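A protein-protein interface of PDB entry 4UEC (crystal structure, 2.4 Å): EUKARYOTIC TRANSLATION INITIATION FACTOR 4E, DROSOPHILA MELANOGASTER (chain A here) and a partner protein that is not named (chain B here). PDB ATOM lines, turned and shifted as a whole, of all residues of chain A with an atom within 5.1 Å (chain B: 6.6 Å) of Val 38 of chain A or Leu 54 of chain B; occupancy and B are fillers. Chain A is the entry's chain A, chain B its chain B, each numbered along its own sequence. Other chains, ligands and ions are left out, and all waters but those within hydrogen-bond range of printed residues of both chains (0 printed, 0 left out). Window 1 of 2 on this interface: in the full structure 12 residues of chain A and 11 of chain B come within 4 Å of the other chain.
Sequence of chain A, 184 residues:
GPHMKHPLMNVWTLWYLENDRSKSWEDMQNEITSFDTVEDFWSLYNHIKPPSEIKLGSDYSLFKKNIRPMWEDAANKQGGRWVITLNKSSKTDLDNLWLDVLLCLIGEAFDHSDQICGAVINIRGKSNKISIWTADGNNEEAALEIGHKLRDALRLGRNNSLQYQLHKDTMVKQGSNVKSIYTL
Of the 12 printed residues of chain A, 6 touch a printed residue of chain B. Along chain A the printed residues that touch a printed residue of chain B span positions 6 to 107. Of the 12 printed residues of chain B, 7 touch a printed residue of chain A. Printed residues of chain B that touch a printed residue of chain A: Tyr 49, Arg 51, Leu 54, Leu 55, Leu 57, Arg 58 and Lys 61. Hydrophobic or aromatic side chains of chain B that line the printed part of chain A: Tyr 49, Leu 54, Leu 55 and Leu 57. Along chain B the printed residues that touch a printed residue of chain A span positions 49 to 61. Among the printed residues, 11 pairs touch across the chains.
O of Leu 55 of chain B lies within hydrogen-bond range of NE of Arg 58 of chain B, 3.0 Å away. The backbone carbonyl oxygen of His 6 of chain A sits at hydrogen-bond distance from the backbone NH of Val 38 of chain A (3.0 Å). NH2 of Arg 58 of chain B is in salt-bridge range of OE2 of Glu 59 of chain B, at 3.5 Å. The side-chain carboxylate of Glu 39 of chain A lies within hydrogen-bond range of a ring nitrogen (ND1) of His 6 of chain A.
Tyr 49 of chain B touches His 6 of chain A (OH to CB, 3.6 Å). His 6 of chain A touches Leu 57 of chain B (CE1 to CD2, 3.6 Å). CG1 of Val 38 of chain A touches CD2 of Leu 54 of chain B (3.6 Å). Leu 57 of chain B touches Val 38 of chain A (CD1 to CG1, 3.7 Å). Leu 55 of chain B touches Trp 42 of chain A (CD2 to CH2, 3.8 Å). CG of Trp 42 of chain A touches CB of Arg 58 of chain B (3.5 Å). Leu 103 of chain A touches Arg 51 of chain B. Leu 103 of chain A touches Leu 54 of chain B.
NZ of Lys 61 of chain B sits at hydrogen-bond distance from O of Glu 39 of chain A (3.2 Å). The backbone carbonyl oxygen (O) of Leu 54 of chain B sits at hydrogen-bond distance from the indole nitrogen (NE1) of Trp 42 of chain A (2.7 Å). The backbone carbonyl oxygen (O) of Gly 107 of chain A lies within hydrogen-bond range of the backbone NH (N) of Tyr 49 of chain B, at 3.1 Å.
Of chain A, only Val 38 (3.6 Å), Trp 42 (2.7 Å) and Leu 103 (3.3 Å) come within 4 Å of Leu 54 of chain B. Of the printed residues of chain B, Trp 42 of chain A touches Leu 54 (2.7 Å), Leu 55 (3.8 Å) and Arg 58 (3.5 Å). Printed residues of chain A within 4 Å of Leu 57 of chain B: His 6 (3.6 Å) and Val 38 (3.7 Å). Of the printed residues of chain A, Tyr 49 of chain B touches His 6 (3.6 Å) and Gly 107 (3.1 Å). Of the printed residues of chain A, Arg 58 of chain B touches Trp 42 (3.5 Å). Gln 56 of chain B touches none of the printed residues of chain A. The nearest printed residue of chain A that does not touch Arg 58 of chain B is Val 38 of chain A (5.6 Å).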
ATOM      1  N   HIS A   6     -14.631 -16.618  -7.071  1.00  0.00           N
ATOM      2  CA  HIS A   6     -15.243 -17.932  -6.900  1.00  0.00           C
ATOM      3  C   HIS A   6     -15.940 -18.020  -5.543  1.00  0.00           C
ATOM      4  O   HIS A   6     -15.276 -17.992  -4.508  1.00  0.00           O
ATOM      5  CB  HIS A   6     -14.190 -19.033  -7.022  1.00  0.00           C
ATOM      6  CG  HIS A   6     -13.528 -19.086  -8.364  1.00  0.00           C
ATOM      7  ND1 HIS A   6     -12.702 -18.084  -8.827  1.00  0.00           N
ATOM      8  CD2 HIS A   6     -13.575 -20.017  -9.346  1.00  0.00           C
ATOM      9  CE1 HIS A   6     -12.267 -18.398 -10.034  1.00  0.00           C
ATOM     10  NE2 HIS A   6     -12.782 -19.566 -10.372  1.00  0.00           N
ATOM     11  N   LEU A   8     -17.858 -19.319  -2.158  1.00  0.00           N
ATOM     12  CA  LEU A   8     -17.848 -20.489  -1.292  1.00  0.00           C
ATOM     13  C   LEU A   8     -19.276 -20.941  -1.007  1.00  0.00           C
ATOM     14  O   LEU A   8     -20.219 -20.161  -1.134  1.00  0.00           O
ATOM     15  CB  LEU A   8     -17.121 -20.182   0.017  1.00  0.00           C
ATOM     16  CG  LEU A   8     -15.687 -19.668  -0.115  1.00  0.00           C
ATOM     17  CD1 LEU A   8     -15.166 -19.206   1.237  1.00  0.00           C
ATOM     18  CD2 LEU A   8     -14.778 -20.740  -0.700  1.00  0.00           C
ATOM     19  N   ASP A  36     -16.679 -14.893   1.820  1.00  0.00           N
ATOM     20  CA  ASP A  36     -17.469 -15.908   1.124  1.00  0.00           C
ATOM     21  C   ASP A  36     -16.983 -16.155  -0.306  1.00  0.00           C
ATOM     22  O   ASP A  36     -17.750 -16.597  -1.163  1.00  0.00           O
ATOM     23  CB  ASP A  36     -18.952 -15.512   1.116  1.00  0.00           C
ATOM     24  CG  ASP A  36     -19.204 -14.154   0.476  1.00  0.00           C
ATOM     25  OD1 ASP A  36     -18.326 -13.648  -0.254  1.00  0.00           O
ATOM     26  OD2 ASP A  36     -20.295 -13.589   0.704  1.00  0.00           O
ATOM     27  N   THR A  37     -15.709 -15.866  -0.557  1.00  0.00           N
ATOM     28  CA  THR A  37     -15.078 -16.195  -1.832  1.00  0.00           C
ATOM     29  C   THR A  37     -13.663 -16.688  -1.580  1.00  0.00           C
ATOM     30  O   THR A  37     -13.062 -16.373  -0.552  1.00  0.00           O
ATOM     31  CB  THR A  37     -15.036 -14.988  -2.792  1.00  0.00           C
ATOM     32  OG1 THR A  37     -14.240 -13.941  -2.221  1.00  0.00           O
ATOM     33  CG2 THR A  37     -16.440 -14.466  -3.071  1.00  0.00           C
ATOM     34  N   VAL A  38     -13.131 -17.465  -2.518  1.00  0.00           N
ATOM     35  CA  VAL A  38     -11.790 -18.016  -2.376  1.00  0.00           C
ATOM     36  C   VAL A  38     -10.748 -16.900  -2.376  1.00  0.00           C
ATOM     37  O   VAL A  38      -9.757 -16.965  -1.648  1.00  0.00           O
ATOM     38  CB  VAL A  38     -11.460 -19.013  -3.504  1.00  0.00           C
ATOM     39  CG1 VAL A  38     -10.087 -19.643  -3.275  1.00  0.00           C
ATOM     40  CG2 VAL A  38     -12.530 -20.093  -3.595  1.00  0.00           C
ATOM     41  N   GLU A  39     -10.979 -15.876  -3.193  1.00  0.00           N
ATOM     42  CA  GLU A  39     -10.036 -14.768  -3.315  1.00  0.00           C
ATOM     43  C   GLU A  39      -9.967 -13.951  -2.028  1.00  0.00           C
ATOM     44  O   GLU A  39      -8.882 -13.558  -1.595  1.00  0.00           O
ATOM     45  CB  GLU A  39     -10.415 -13.863  -4.489  1.00  0.00           C
ATOM     46  CG  GLU A  39     -10.159 -14.478  -5.865  1.00  0.00           C
ATOM     47  CD  GLU A  39     -11.205 -15.505  -6.269  1.00  0.00           C
ATOM     48  OE1 GLU A  39     -12.052 -15.868  -5.427  1.00  0.00           O
ATOM     49  OE2 GLU A  39     -11.181 -15.948  -7.436  1.00  0.00           O
ATOM     50  N   ASP A  40     -11.121 -13.698  -1.418  1.00  0.00           N
ATOM     51  CA  ASP A  40     -11.172 -12.936  -0.173  1.00  0.00           C
ATOM     52  C   ASP A  40     -10.599 -13.733   0.999  1.00  0.00           C
ATOM     53  O   ASP A  40     -10.147 -13.152   1.987  1.00  0.00           O
ATOM     54  CB  ASP A  40     -12.608 -12.512   0.139  1.00  0.00           C
ATOM     55  CG  ASP A  40     -13.131 -11.463  -0.824  1.00  0.00           C
ATOM     56  OD1 ASP A  40     -12.335 -10.605  -1.266  1.00  0.00           O
ATOM     57  OD2 ASP A  40     -14.338 -11.496  -1.138  1.00  0.00           O
ATOM     58  N   PHE A  41     -10.624 -15.060   0.894  1.00  0.00           N
ATOM     59  CA  PHE A  41      -9.987 -15.900   1.902  1.00  0.00           C
ATOM     60  C   PHE A  41      -8.476 -15.712   1.873  1.00  0.00           C
ATOM     61  O   PHE A  41      -7.856 -15.466   2.907  1.00  0.00           O
ATOM     62  CB  PHE A  41     -10.322 -17.379   1.694  1.00  0.00           C
ATOM     63  CG  PHE A  41      -9.366 -18.309   2.385  1.00  0.00           C
ATOM     64  CD1 PHE A  41      -9.488 -18.568   3.740  1.00  0.00           C
ATOM     65  CD2 PHE A  41      -8.331 -18.909   1.685  1.00  0.00           C
ATOM     66  CE1 PHE A  41      -8.601 -19.415   4.380  1.00  0.00           C
ATOM     67  CE2 PHE A  41      -7.442 -19.755   2.322  1.00  0.00           C
ATOM     68  CZ  PHE A  41      -7.575 -20.007   3.670  1.00  0.00           C
ATOM     69  N   TRP A  42      -7.888 -15.835   0.685  1.00  0.00           N
ATOM     70  CA  TRP A  42      -6.442 -15.697   0.529  1.00  0.00           C
ATOM     71  C   TRP A  42      -5.982 -14.292   0.899  1.00  0.00           C
ATOM     72  O   TRP A  42      -4.925 -14.119   1.502  1.00  0.00           O
ATOM     73  CB  TRP A  42      -6.016 -16.020  -0.906  1.00  0.00           C
ATOM     74  CG  TRP A  42      -6.079 -17.478  -1.239  1.00  0.00           C
ATOM     75  CD1 TRP A  42      -6.855 -18.068  -2.194  1.00  0.00           C
ATOM     76  CD2 TRP A  42      -5.339 -18.534  -0.614  1.00  0.00           C
ATOM     77  NE1 TRP A  42      -6.639 -19.426  -2.207  1.00  0.00           N
ATOM     78  CE2 TRP A  42      -5.716 -19.737  -1.243  1.00  0.00           C
ATOM     79  CE3 TRP A  42      -4.393 -18.577   0.415  1.00  0.00           C
ATOM     80  CZ2 TRP A  42      -5.179 -20.968  -0.877  1.00  0.00           C
ATOM     81  CZ3 TRP A  42      -3.864 -19.800   0.778  1.00  0.00           C
ATOM     82  CH2 TRP A  42      -4.258 -20.979   0.133  1.00  0.00           C
ATOM     83  N   LEU A 103      -8.611 -25.142   4.205  1.00  0.00           N
ATOM     84  CA  LEU A 103      -8.969 -25.419   2.817  1.00  0.00           C
ATOM     85  C   LEU A 103     -10.015 -26.528   2.722  1.00  0.00           C
ATOM     86  O   LEU A 103     -10.860 -26.516   1.826  1.00  0.00           O
ATOM     87  CB  LEU A 103      -7.724 -25.794   2.005  1.00  0.00           C
ATOM     88  CG  LEU A 103      -6.666 -24.696   1.859  1.00  0.00           C
ATOM     89  CD1 LEU A 103      -5.430 -25.231   1.149  1.00  0.00           C
ATOM     90  CD2 LEU A 103      -7.220 -23.486   1.120  1.00  0.00           C
ATOM     91  N   ILE A 106     -13.456 -24.523   3.763  1.00  0.00           N
ATOM     92  CA  ILE A 106     -14.002 -23.596   2.774  1.00  0.00           C
ATOM     93  C   ILE A 106     -14.258 -24.302   1.447  1.00  0.00           C
ATOM     94  O   ILE A 106     -15.095 -23.867   0.654  1.00  0.00           O
ATOM     95  CB  ILE A 106     -13.069 -22.380   2.547  1.00  0.00           C
ATOM     96  CG1 ILE A 106     -11.775 -22.790   1.836  1.00  0.00           C
ATOM     97  CG2 ILE A 106     -12.773 -21.693   3.877  1.00  0.00           C
ATOM     98  CD1 ILE A 106     -10.881 -21.622   1.491  1.00  0.00           C
ATOM     99  N   GLY A 107     -13.540 -25.395   1.214  1.00  0.00           N
ATOM    100  CA  GLY A 107     -13.715 -26.185   0.009  1.00  0.00           C
ATOM    101  C   GLY A 107     -14.838 -27.202   0.119  1.00  0.00           C
ATOM    102  O   GLY A 107     -15.205 -27.827  -0.875  1.00  0.00           O
ATOM    103  N   TYR B  49     -14.413 -27.205  -3.773  1.00  0.00           N
ATOM    104  CA  TYR B  49     -13.079 -27.011  -4.344  1.00  0.00           C
ATOM    105  C   TYR B  49     -12.027 -27.921  -3.716  1.00  0.00           C
ATOM    106  O   TYR B  49     -11.972 -28.077  -2.496  1.00  0.00           O
ATOM    107  CB  TYR B  49     -12.644 -25.552  -4.179  1.00  0.00           C
ATOM    108  CG  TYR B  49     -13.634 -24.542  -4.714  1.00  0.00           C
ATOM    109  CD1 TYR B  49     -13.582 -24.121  -6.037  1.00  0.00           C
ATOM    110  CD2 TYR B  49     -14.616 -24.004  -3.893  1.00  0.00           C
ATOM    111  CE1 TYR B  49     -14.485 -23.195  -6.528  1.00  0.00           C
ATOM    112  CE2 TYR B  49     -15.522 -23.077  -4.375  1.00  0.00           C
ATOM    113  CZ  TYR B  49     -15.453 -22.677  -5.692  1.00  0.00           C
ATOM    114  OH  TYR B  49     -16.356 -21.754  -6.172  1.00  0.00           O
ATOM    115  N   ASP B  50     -11.185 -28.509  -4.562  1.00  0.00           N
ATOM    116  CA  ASP B  50     -10.055 -29.311  -4.104  1.00  0.00           C
ATOM    117  C   ASP B  50      -9.020 -28.436  -3.408  1.00  0.00           C
ATOM    118  O   ASP B  50      -9.136 -27.211  -3.395  1.00  0.00           O
ATOM    119  CB  ASP B  50      -9.391 -30.040  -5.276  1.00  0.00           C
ATOM    120  CG  ASP B  50     -10.325 -31.005  -5.972  1.00  0.00           C
ATOM    121  OD1 ASP B  50     -11.074 -31.721  -5.274  1.00  0.00           O
ATOM    122  OD2 ASP B  50     -10.309 -31.048  -7.221  1.00  0.00           O
ATOM    123  N   ARG B  51      -8.003 -29.068  -2.837  1.00  0.00           N
ATOM    124  CA  ARG B  51      -6.875 -28.331  -2.287  1.00  0.00           C
ATOM    125  C   ARG B  51      -6.136 -27.615  -3.411  1.00  0.00           C
ATOM    126  O   ARG B  51      -5.859 -26.418  -3.324  1.00  0.00           O
ATOM    127  CB  ARG B  51      -5.923 -29.265  -1.542  1.00  0.00           C
ATOM    128  CG  ARG B  51      -4.716 -28.563  -0.943  1.00  0.00           C
ATOM    129  CD  ARG B  51      -3.784 -29.545  -0.263  1.00  0.00           C
ATOM    130  NE  ARG B  51      -2.578 -28.893   0.243  1.00  0.00           N
ATOM    131  CZ  ARG B  51      -1.502 -28.620  -0.493  1.00  0.00           C
ATOM    132  NH1 ARG B  51      -1.469 -28.935  -1.784  1.00  0.00           N
ATOM    133  NH2 ARG B  51      -0.456 -28.027   0.063  1.00  0.00           N
ATOM    134  N   GLU B  52      -5.827 -28.356  -4.469  1.00  0.00           N
ATOM    135  CA  GLU B  52      -5.047 -27.821  -5.579  1.00  0.00           C
ATOM    136  C   GLU B  52      -5.777 -26.691  -6.291  1.00  0.00           C
ATOM    137  O   GLU B  52      -5.162 -25.703  -6.689  1.00  0.00           O
ATOM    138  CB  GLU B  52      -4.713 -28.929  -6.575  1.00  0.00           C
ATOM    139  CG  GLU B  52      -3.933 -30.083  -5.966  1.00  0.00           C
ATOM    140  CD  GLU B  52      -3.518 -31.107  -6.999  1.00  0.00           C
ATOM    141  OE1 GLU B  52      -3.563 -30.782  -8.204  1.00  0.00           O
ATOM    142  OE2 GLU B  52      -3.149 -32.234  -6.606  1.00  0.00           O
ATOM    143  N   GLN B  53      -7.088 -26.837  -6.450  1.00  0.00           N
ATOM    144  CA  GLN B  53      -7.896 -25.802  -7.083  1.00  0.00           C
ATOM    145  C   GLN B  53      -7.876 -24.521  -6.258  1.00  0.00           C
ATOM    146  O   GLN B  53      -7.707 -23.429  -6.797  1.00  0.00           O
ATOM    147  CB  GLN B  53      -9.335 -26.282  -7.273  1.00  0.00           C
ATOM    148  CG  GLN B  53      -9.488 -27.386  -8.304  1.00  0.00           C
ATOM    149  CD  GLN B  53     -10.921 -27.867  -8.431  1.00  0.00           C
ATOM    150  OE1 GLN B  53     -11.696 -27.802  -7.477  1.00  0.00           O
ATOM    151  NE2 GLN B  53     -11.281 -28.348  -9.616  1.00  0.00           N
ATOM    152  N   LEU B  54      -8.046 -24.661  -4.947  1.00  0.00           N
ATOM    153  CA  LEU B  54      -8.017 -23.517  -4.044  1.00  0.00           C
ATOM    154  C   LEU B  54      -6.650 -22.838  -4.060  1.00  0.00           C
ATOM    155  O   LEU B  54      -6.547 -21.633  -3.829  1.00  0.00           O
ATOM    156  CB  LEU B  54      -8.370 -23.951  -2.619  1.00  0.00           C
ATOM    157  CG  LEU B  54      -9.836 -24.308  -2.364  1.00  0.00           C
ATOM    158  CD1 LEU B  54      -9.990 -25.021  -1.024  1.00  0.00           C
ATOM    159  CD2 LEU B  54     -10.706 -23.065  -2.408  1.00  0.00           C
ATOM    160  N   LEU B  55      -5.606 -23.617  -4.334  1.00  0.00           N
ATOM    161  CA  LEU B  55      -4.245 -23.090  -4.388  1.00  0.00           C
ATOM    162  C   LEU B  55      -3.979 -22.350  -5.693  1.00  0.00           C
ATOM    163  O   LEU B  55      -3.198 -21.406  -5.723  1.00  0.00           O
ATOM    164  CB  LEU B  55      -3.226 -24.219  -4.217  1.00  0.00           C
ATOM    165  CG  LEU B  55      -3.039 -24.778  -2.805  1.00  0.00           C
ATOM    166  CD1 LEU B  55      -2.069 -25.952  -2.833  1.00  0.00           C
ATOM    167  CD2 LEU B  55      -2.545 -23.708  -1.844  1.00  0.00           C
ATOM    168  N   GLN B  56      -4.627 -22.781  -6.769  1.00  0.00           N
ATOM    169  CA  GLN B  56      -4.483 -22.122  -8.065  1.00  0.00           C
ATOM    170  C   GLN B  56      -5.025 -20.695  -8.048  1.00  0.00           C
ATOM    171  O   GLN B  56      -4.567 -19.841  -8.808  1.00  0.00           O
ATOM    172  CB  GLN B  56      -5.207 -22.919  -9.152  1.00  0.00           C
ATOM    173  CG  GLN B  56      -4.526 -24.222  -9.548  1.00  0.00           C
ATOM    174  CD  GLN B  56      -5.455 -25.175 -10.289  1.00  0.00           C
ATOM    175  OE1 GLN B  56      -6.673 -25.003 -10.286  1.00  0.00           O
ATOM    176  NE2 GLN B  56      -4.877 -26.186 -10.929  1.00  0.00           N
ATOM    177  N   LEU B  57      -5.998 -20.441  -7.178  1.00  0.00           N
ATOM    178  CA  LEU B  57      -6.742 -19.184  -7.203  1.00  0.00           C
ATOM    179  C   LEU B  57      -6.079 -18.060  -6.403  1.00  0.00           C
ATOM    180  O   LEU B  57      -6.423 -16.890  -6.572  1.00  0.00           O
ATOM    181  CB  LEU B  57      -8.161 -19.424  -6.685  1.00  0.00           C
ATOM    182  CG  LEU B  57      -9.000 -20.398  -7.520  1.00  0.00           C
ATOM    183  CD1 LEU B  57     -10.352 -20.651  -6.864  1.00  0.00           C
ATOM    184  CD2 LEU B  57      -9.189 -19.890  -8.945  1.00  0.00           C
ATOM    185  N   ARG B  58      -5.132 -18.409  -5.539  1.00  0.00           N
ATOM    186  CA  ARG B  58      -4.383 -17.409  -4.786  1.00  0.00           C
ATOM    187  C   ARG B  58      -3.385 -16.693  -5.691  1.00  0.00           C
ATOM    188  O   ARG B  58      -3.103 -15.507  -5.521  1.00  0.00           O
ATOM    189  CB  ARG B  58      -3.638 -18.064  -3.618  1.00  0.00           C
ATOM    190  CG  ARG B  58      -2.354 -18.759  -4.042  1.00  0.00           C
ATOM    191  CD  ARG B  58      -1.840 -19.761  -3.019  1.00  0.00           C
ATOM    192  NE  ARG B  58      -1.097 -20.834  -3.684  1.00  0.00           N
ATOM    193  CZ  ARG B  58       0.064 -21.342  -3.271  1.00  0.00           C
ATOM    194  NH1 ARG B  58       0.660 -20.897  -2.171  1.00  0.00           N
ATOM    195  NH2 ARG B  58       0.635 -22.315  -3.969  1.00  0.00           N
ATOM    196  N   GLU B  59      -2.867 -17.438  -6.662  1.00  0.00           N
ATOM    197  CA  GLU B  59      -1.667 -17.054  -7.395  1.00  0.00           C
ATOM    198  C   GLU B  59      -1.858 -15.870  -8.333  1.00  0.00           C
ATOM    199  O   GLU B  59      -0.882 -15.289  -8.806  1.00  0.00           O
ATOM    200  CB  GLU B  59      -1.159 -18.259  -8.193  1.00  0.00           C
ATOM    201  CG  GLU B  59      -0.564 -19.363  -7.328  1.00  0.00           C
ATOM    202  CD  GLU B  59      -0.548 -20.715  -8.020  1.00  0.00           C
ATOM    203  OE1 GLU B  59      -0.708 -20.754  -9.259  1.00  0.00           O
ATOM    204  OE2 GLU B  59      -0.382 -21.739  -7.321  1.00  0.00           O
ATOM    205  N   LYS B  61      -2.914 -12.892  -7.781  1.00  0.00           N
ATOM    206  CA  LYS B  61      -2.551 -11.603  -7.200  1.00  0.00           C
ATOM    207  C   LYS B  61      -1.038 -11.447  -7.043  1.00  0.00           C
ATOM    208  O   LYS B  61      -0.481 -10.400  -7.370  1.00  0.00           O
ATOM    209  CB  LYS B  61      -3.231 -11.415  -5.841  1.00  0.00           C
ATOM    210  CG  LYS B  61      -4.753 -11.482  -5.885  1.00  0.00           C
ATOM    211  CD  LYS B  61      -5.380 -10.627  -4.787  1.00  0.00           C
ATOM    212  CE  LYS B  61      -6.707 -11.199  -4.294  1.00  0.00           C
ATOM    213  NZ  LYS B  61      -6.528 -12.462  -3.518  1.00  0.00           N
